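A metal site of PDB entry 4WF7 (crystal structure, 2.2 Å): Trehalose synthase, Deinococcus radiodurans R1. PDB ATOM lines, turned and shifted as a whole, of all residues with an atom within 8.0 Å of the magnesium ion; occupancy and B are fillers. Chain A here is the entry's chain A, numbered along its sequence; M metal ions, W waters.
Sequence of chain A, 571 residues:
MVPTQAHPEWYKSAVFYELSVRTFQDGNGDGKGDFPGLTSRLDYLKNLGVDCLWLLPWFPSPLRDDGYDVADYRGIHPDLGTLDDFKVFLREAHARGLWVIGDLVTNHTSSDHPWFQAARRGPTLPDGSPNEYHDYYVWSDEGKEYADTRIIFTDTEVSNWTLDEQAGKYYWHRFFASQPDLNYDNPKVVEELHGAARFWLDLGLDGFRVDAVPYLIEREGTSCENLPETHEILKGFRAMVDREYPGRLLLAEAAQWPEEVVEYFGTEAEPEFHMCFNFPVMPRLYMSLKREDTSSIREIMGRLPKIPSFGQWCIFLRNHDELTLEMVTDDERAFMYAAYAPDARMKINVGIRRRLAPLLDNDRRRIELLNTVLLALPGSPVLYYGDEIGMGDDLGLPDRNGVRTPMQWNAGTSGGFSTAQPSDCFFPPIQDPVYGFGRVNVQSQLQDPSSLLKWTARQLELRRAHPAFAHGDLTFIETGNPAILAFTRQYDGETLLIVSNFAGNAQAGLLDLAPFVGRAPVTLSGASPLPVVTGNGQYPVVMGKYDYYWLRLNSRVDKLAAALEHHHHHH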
ATOM      1  N   VAL A  21      17.600  34.686  -8.524  1.00  0.00           N
ATOM      2  CA  VAL A  21      16.781  33.934  -7.576  1.00  0.00           C
ATOM      3  C   VAL A  21      16.939  32.448  -7.785  1.00  0.00           C
ATOM      4  O   VAL A  21      17.020  31.693  -6.836  1.00  0.00           O
ATOM      5  CB  VAL A  21      15.283  34.280  -7.678  1.00  0.00           C
ATOM      6  CG1 VAL A  21      14.479  33.399  -6.755  1.00  0.00           C
ATOM      7  CG2 VAL A  21      15.043  35.752  -7.362  1.00  0.00           C
ATOM      8  N   ARG A  22      17.004  32.018  -9.038  1.00  0.00           N
ATOM      9  CA  ARG A  22      17.146  30.600  -9.349  1.00  0.00           C
ATOM     10  C   ARG A  22      18.458  29.980  -8.849  1.00  0.00           C
ATOM     11  O   ARG A  22      18.605  28.756  -8.830  1.00  0.00           O
ATOM     12  CB  ARG A  22      17.046  30.387 -10.852  1.00  0.00           C
ATOM     13  CG  ARG A  22      16.840  28.957 -11.257  1.00  0.00           C
ATOM     14  CD  ARG A  22      16.584  28.861 -12.757  1.00  0.00           C
ATOM     15  NE  ARG A  22      15.234  29.307 -13.080  1.00  0.00           N
ATOM     16  CZ  ARG A  22      14.917  30.498 -13.572  1.00  0.00           C
ATOM     17  NH1 ARG A  22      15.844  31.432 -13.784  1.00  0.00           N
ATOM     18  NH2 ARG A  22      13.630  30.756 -13.836  1.00  0.00           N
ATOM     19  N   GLN A  25      19.010  30.528  -3.331  1.00  0.00           N
ATOM     20  CA  GLN A  25      18.604  29.561  -2.318  1.00  0.00           C
ATOM     21  C   GLN A  25      17.364  28.796  -2.748  1.00  0.00           C
ATOM     22  O   GLN A  25      16.314  29.394  -3.008  1.00  0.00           O
ATOM     23  CB  GLN A  25      18.330  30.271  -1.002  1.00  0.00           C
ATOM     24  CG  GLN A  25      17.910  29.363   0.140  1.00  0.00           C
ATOM     25  CD  GLN A  25      19.012  28.415   0.549  1.00  0.00           C
ATOM     26  OE1 GLN A  25      20.098  28.848   0.953  1.00  0.00           O
ATOM     27  NE2 GLN A  25      18.769  27.129   0.422  1.00  0.00           N
ATOM     28  N   ASP A  26      17.484  27.470  -2.799  1.00  0.00           N
ATOM     29  CA  ASP A  26      16.381  26.593  -3.114  1.00  0.00           C
ATOM     30  C   ASP A  26      15.657  26.358  -1.811  1.00  0.00           C
ATOM     31  O   ASP A  26      16.254  25.901  -0.859  1.00  0.00           O
ATOM     32  CB  ASP A  26      16.933  25.267  -3.620  1.00  0.00           C
ATOM     33  CG  ASP A  26      15.872  24.218  -3.892  1.00  0.00           C
ATOM     34  OD1 ASP A  26      14.671  24.522  -3.880  1.00  0.00           O
ATOM     35  OD2 ASP A  26      16.279  23.062  -4.128  1.00  0.00           O
ATOM     36  N   GLY A  27      14.366  26.695  -1.773  1.00  0.00           N
ATOM     37  CA  GLY A  27      13.559  26.477  -0.603  1.00  0.00           C
ATOM     38  C   GLY A  27      12.716  25.211  -0.661  1.00  0.00           C
ATOM     39  O   GLY A  27      11.926  24.992   0.243  1.00  0.00           O
ATOM     40  N   ASN A  28      12.847  24.377  -1.706  1.00  0.00           N
ATOM     41  CA  ASN A  28      11.941  23.197  -1.815  1.00  0.00           C
ATOM     42  C   ASN A  28      12.536  21.918  -2.363  1.00  0.00           C
ATOM     43  O   ASN A  28      11.798  21.008  -2.762  1.00  0.00           O
ATOM     44  CB  ASN A  28      10.649  23.562  -2.569  1.00  0.00           C
ATOM     45  CG  ASN A  28      10.880  23.775  -4.058  1.00  0.00           C
ATOM     46  OD1 ASN A  28      11.961  24.145  -4.498  1.00  0.00           O
ATOM     47  ND2 ASN A  28       9.858  23.515  -4.847  1.00  0.00           N
ATOM     48  N   GLY A  29      13.861  21.824  -2.333  1.00  0.00           N
ATOM     49  CA  GLY A  29      14.568  20.594  -2.703  1.00  0.00           C
ATOM     50  C   GLY A  29      14.586  20.221  -4.181  1.00  0.00           C
ATOM     51  O   GLY A  29      15.036  19.131  -4.514  1.00  0.00           O
ATOM     52  N   ASP A  30      14.114  21.071  -5.075  1.00  0.00           N
ATOM     53  CA  ASP A  30      14.071  20.654  -6.486  1.00  0.00           C
ATOM     54  C   ASP A  30      15.346  21.078  -7.247  1.00  0.00           C
ATOM     55  O   ASP A  30      15.434  20.871  -8.434  1.00  0.00           O
ATOM     56  CB  ASP A  30      12.778  21.124  -7.203  1.00  0.00           C
ATOM     57  CG  ASP A  30      12.719  22.633  -7.403  1.00  0.00           C
ATOM     58  OD1 ASP A  30      13.583  23.364  -6.896  1.00  0.00           O
ATOM     59  OD2 ASP A  30      11.760  23.113  -8.023  1.00  0.00           O
ATOM     60  N   GLY A  31      16.334  21.659  -6.570  1.00  0.00           N
ATOM     61  CA  GLY A  31      17.588  22.086  -7.228  1.00  0.00           C
ATOM     62  C   GLY A  31      17.522  23.463  -7.873  1.00  0.00           C
ATOM     63  O   GLY A  31      18.524  23.941  -8.395  1.00  0.00           O
ATOM     64  N   LYS A  32      16.350  24.089  -7.857  1.00  0.00           N
ATOM     65  CA  LYS A  32      16.191  25.473  -8.339  1.00  0.00           C
ATOM     66  C   LYS A  32      15.994  26.449  -7.205  1.00  0.00           C
ATOM     67  O   LYS A  32      15.104  26.261  -6.381  1.00  0.00           O
ATOM     68  CB  LYS A  32      14.976  25.588  -9.256  1.00  0.00           C
ATOM     69  CG  LYS A  32      15.175  24.934 -10.606  1.00  0.00           C
ATOM     70  CD  LYS A  32      13.910  24.213 -11.039  1.00  0.00           C
ATOM     71  CE  LYS A  32      14.106  23.442 -12.331  1.00  0.00           C
ATOM     72  NZ  LYS A  32      12.868  23.567 -13.152  1.00  0.00           N
ATOM     73  N   GLY A  33      16.782  27.501  -7.175  1.00  0.00           N
ATOM     74  CA  GLY A  33      16.543  28.626  -6.245  1.00  0.00           C
ATOM     75  C   GLY A  33      15.168  29.224  -6.440  1.00  0.00           C
ATOM     76  O   GLY A  33      14.584  29.144  -7.552  1.00  0.00           O
ATOM     77  N   ASP A  34      14.614  29.788  -5.372  1.00  0.00           N
ATOM     78  CA  ASP A  34      13.249  30.266  -5.428  1.00  0.00           C
ATOM     79  C   ASP A  34      13.005  31.340  -4.414  1.00  0.00           C
ATOM     80  O   ASP A  34      13.878  31.676  -3.593  1.00  0.00           O
ATOM     81  CB  ASP A  34      12.235  29.108  -5.273  1.00  0.00           C
ATOM     82  CG  ASP A  34      12.467  28.269  -4.032  1.00  0.00           C
ATOM     83  OD1 ASP A  34      12.378  28.817  -2.916  1.00  0.00           O
ATOM     84  OD2 ASP A  34      12.781  27.069  -4.172  1.00  0.00           O
ATOM     85  N   PHE A  35      11.843  31.963  -4.528  1.00  0.00           N
ATOM     86  CA  PHE A  35      11.555  33.117  -3.684  1.00  0.00           C
ATOM     87  C   PHE A  35      11.457  32.767  -2.181  1.00  0.00           C
ATOM     88  O   PHE A  35      11.965  33.517  -1.366  1.00  0.00           O
ATOM     89  CB  PHE A  35      10.299  33.865  -4.174  1.00  0.00           C
ATOM     90  CG  PHE A  35      10.578  34.858  -5.262  1.00  0.00           C
ATOM     91  CD1 PHE A  35      11.203  36.055  -4.967  1.00  0.00           C
ATOM     92  CD2 PHE A  35      10.243  34.589  -6.568  1.00  0.00           C
ATOM     93  CE1 PHE A  35      11.458  36.990  -5.956  1.00  0.00           C
ATOM     94  CE2 PHE A  35      10.499  35.515  -7.568  1.00  0.00           C
ATOM     95  CZ  PHE A  35      11.087  36.726  -7.257  1.00  0.00           C
ATOM     96  N   PRO A  36      10.820  31.633  -1.826  1.00  0.00           N
ATOM     97  CA  PRO A  36      10.794  31.270  -0.396  1.00  0.00           C
ATOM     98  C   PRO A  36      12.202  31.092   0.182  1.00  0.00           C
ATOM     99  O   PRO A  36      12.475  31.502   1.329  1.00  0.00           O
ATOM    100  CB  PRO A  36      10.014  29.959  -0.390  1.00  0.00           C
ATOM    101  CG  PRO A  36       9.119  30.063  -1.565  1.00  0.00           C
ATOM    102  CD  PRO A  36       9.924  30.769  -2.616  1.00  0.00           C
ATOM    103  N   GLY A  37      13.082  30.497  -0.618  1.00  0.00           N
ATOM    104  CA  GLY A  37      14.503  30.335  -0.303  1.00  0.00           C
ATOM    105  C   GLY A  37      15.181  31.681  -0.170  1.00  0.00           C
ATOM    106  O   GLY A  37      15.905  31.923   0.789  1.00  0.00           O
ATOM    107  N   PRO A  78       7.570  29.672 -12.914  1.00  0.00           N
ATOM    108  CA  PRO A  78       7.179  28.602 -11.989  1.00  0.00           C
ATOM    109  C   PRO A  78       8.323  27.971 -11.177  1.00  0.00           C
ATOM    110  O   PRO A  78       8.081  27.480 -10.077  1.00  0.00           O
ATOM    111  CB  PRO A  78       6.538  27.549 -12.885  1.00  0.00           C
ATOM    112  CG  PRO A  78       6.247  28.219 -14.165  1.00  0.00           C
ATOM    113  CD  PRO A  78       7.085  29.437 -14.294  1.00  0.00           C
ATOM    114  N   ASP A  79       9.539  27.936 -11.712  1.00  0.00           N
ATOM    115  CA  ASP A  79      10.710  27.547 -10.921  1.00  0.00           C
ATOM    116  C   ASP A  79      10.796  28.336  -9.627  1.00  0.00           C
ATOM    117  O   ASP A  79      11.248  27.815  -8.612  1.00  0.00           O
ATOM    118  CB  ASP A  79      12.026  27.819 -11.665  1.00  0.00           C
ATOM    119  CG  ASP A  79      12.234  26.956 -12.863  1.00  0.00           C
ATOM    120  OD1 ASP A  79      11.416  26.035 -13.091  1.00  0.00           O
ATOM    121  OD2 ASP A  79      13.246  27.172 -13.566  1.00  0.00           O
ATOM    122  N   LEU A  80      10.396  29.587  -9.641  1.00  0.00           N
ATOM    123  CA  LEU A  80      10.691  30.465  -8.528  1.00  0.00           C
ATOM    124  C   LEU A  80       9.575  30.584  -7.483  1.00  0.00           C
ATOM    125  O   LEU A  80       9.726  31.291  -6.486  1.00  0.00           O
ATOM    126  CB  LEU A  80      11.062  31.843  -9.036  1.00  0.00           C
ATOM    127  CG  LEU A  80      12.013  31.875 -10.234  1.00  0.00           C
ATOM    128  CD1 LEU A  80      12.245  33.319 -10.663  1.00  0.00           C
ATOM    129  CD2 LEU A  80      13.332  31.170  -9.935  1.00  0.00           C
ATOM    130  N   GLY A  81       8.469  29.869  -7.697  1.00  0.00           N
ATOM    131  CA  GLY A  81       7.306  29.952  -6.811  1.00  0.00           C
ATOM    132  C   GLY A  81       6.163  30.683  -7.484  1.00  0.00           C
ATOM    133  O   GLY A  81       5.973  30.567  -8.695  1.00  0.00           O
ATOM    134  N   PHE A 417      23.023  25.331  -0.721  1.00  0.00           N
ATOM    135  CA  PHE A 417      22.081  25.894  -1.684  1.00  0.00           C
ATOM    136  C   PHE A 417      20.796  25.095  -1.798  1.00  0.00           C
ATOM    137  O   PHE A 417      19.730  25.689  -2.026  1.00  0.00           O
ATOM    138  CB  PHE A 417      22.732  25.956  -3.070  1.00  0.00           C
ATOM    139  CG  PHE A 417      21.772  26.146  -4.172  1.00  0.00           C
ATOM    140  CD1 PHE A 417      21.148  27.343  -4.373  1.00  0.00           C
ATOM    141  CD2 PHE A 417      21.530  25.111  -5.064  1.00  0.00           C
ATOM    142  CE1 PHE A 417      20.275  27.537  -5.428  1.00  0.00           C
ATOM    143  CE2 PHE A 417      20.648  25.279  -6.114  1.00  0.00           C
ATOM    144  CZ  PHE A 417      20.018  26.488  -6.298  1.00  0.00           C
ATOM    145  N   SER A 418      20.902  23.780  -1.649  1.00  0.00           N
ATOM    146  CA  SER A 418      19.780  22.890  -1.818  1.00  0.00           C
ATOM    147  C   SER A 418      20.026  21.572  -1.116  1.00  0.00           C
ATOM    148  O   SER A 418      21.174  21.147  -0.981  1.00  0.00           O
ATOM    149  CB  SER A 418      19.575  22.591  -3.313  1.00  0.00           C
ATOM    150  OG  SER A 418      18.559  21.634  -3.504  1.00  0.00           O
HETATM  151 MG    MG M   1      13.317  25.327  -5.459  1.00  0.00          MG
HETATM  152  O   HOH W   1      11.678  25.589  -6.924  1.00  0.00           O
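The magnesium ion is bound by OD1 of Asn 28 (2.0 Å), water W1 (2.2 Å), O of Lys 32 (2.2 Å), OD1 of Asp 26 (2.2 Å), OD2 of Asp 34 (2.2 Å) and OD1 of Asp 30 (2.4 Å).
The magnesium ion has six donor atoms within binding distance.
Within 4 Å of the magnesium ion: Asp 26, Asn 28, Asp 30, Lys 32 and Asp 34.
The side-chain carboxylate of Asp 79 is in salt-bridge range of the side-chain amino group of Lys 32 (2.9 Å).
The side-chain carboxylate (OD2) of Asp 26 lies within hydrogen-bond range of the backbone NH (N) of Gly 31.
N of Gly 37 lies within hydrogen-bond range of OD1 of Asp 34 (2.9 Å).
The side-chain carboxylate (OD2) of Asp 26 lies within hydrogen-bond range of the side-chain hydroxyl (OG) of Ser 418 (2.8 Å).
The backbone NH (N) of Asp 34 is in hydrogen-bond range of the backbone carbonyl oxygen (O) of Val 21 (3.4 Å).
The backbone NH (N) of Asp 26 lies within hydrogen-bond range of the backbone carbonyl oxygen (O) of Phe 417 (3.0 Å).
O of Gln 25 is in hydrogen-bond range of N of Asp 34.
The side-chain carboxylate (OD1) of Asp 34 sits at hydrogen-bond distance from the backbone NH (N) of Gly 27 (3.1 Å).
Water W1 lies within hydrogen-bond range of OD2 of Asp 30 (2.7 Å), O of Asp 79 (2.8 Å) and ND2 of Asn 28 (3.5 Å).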
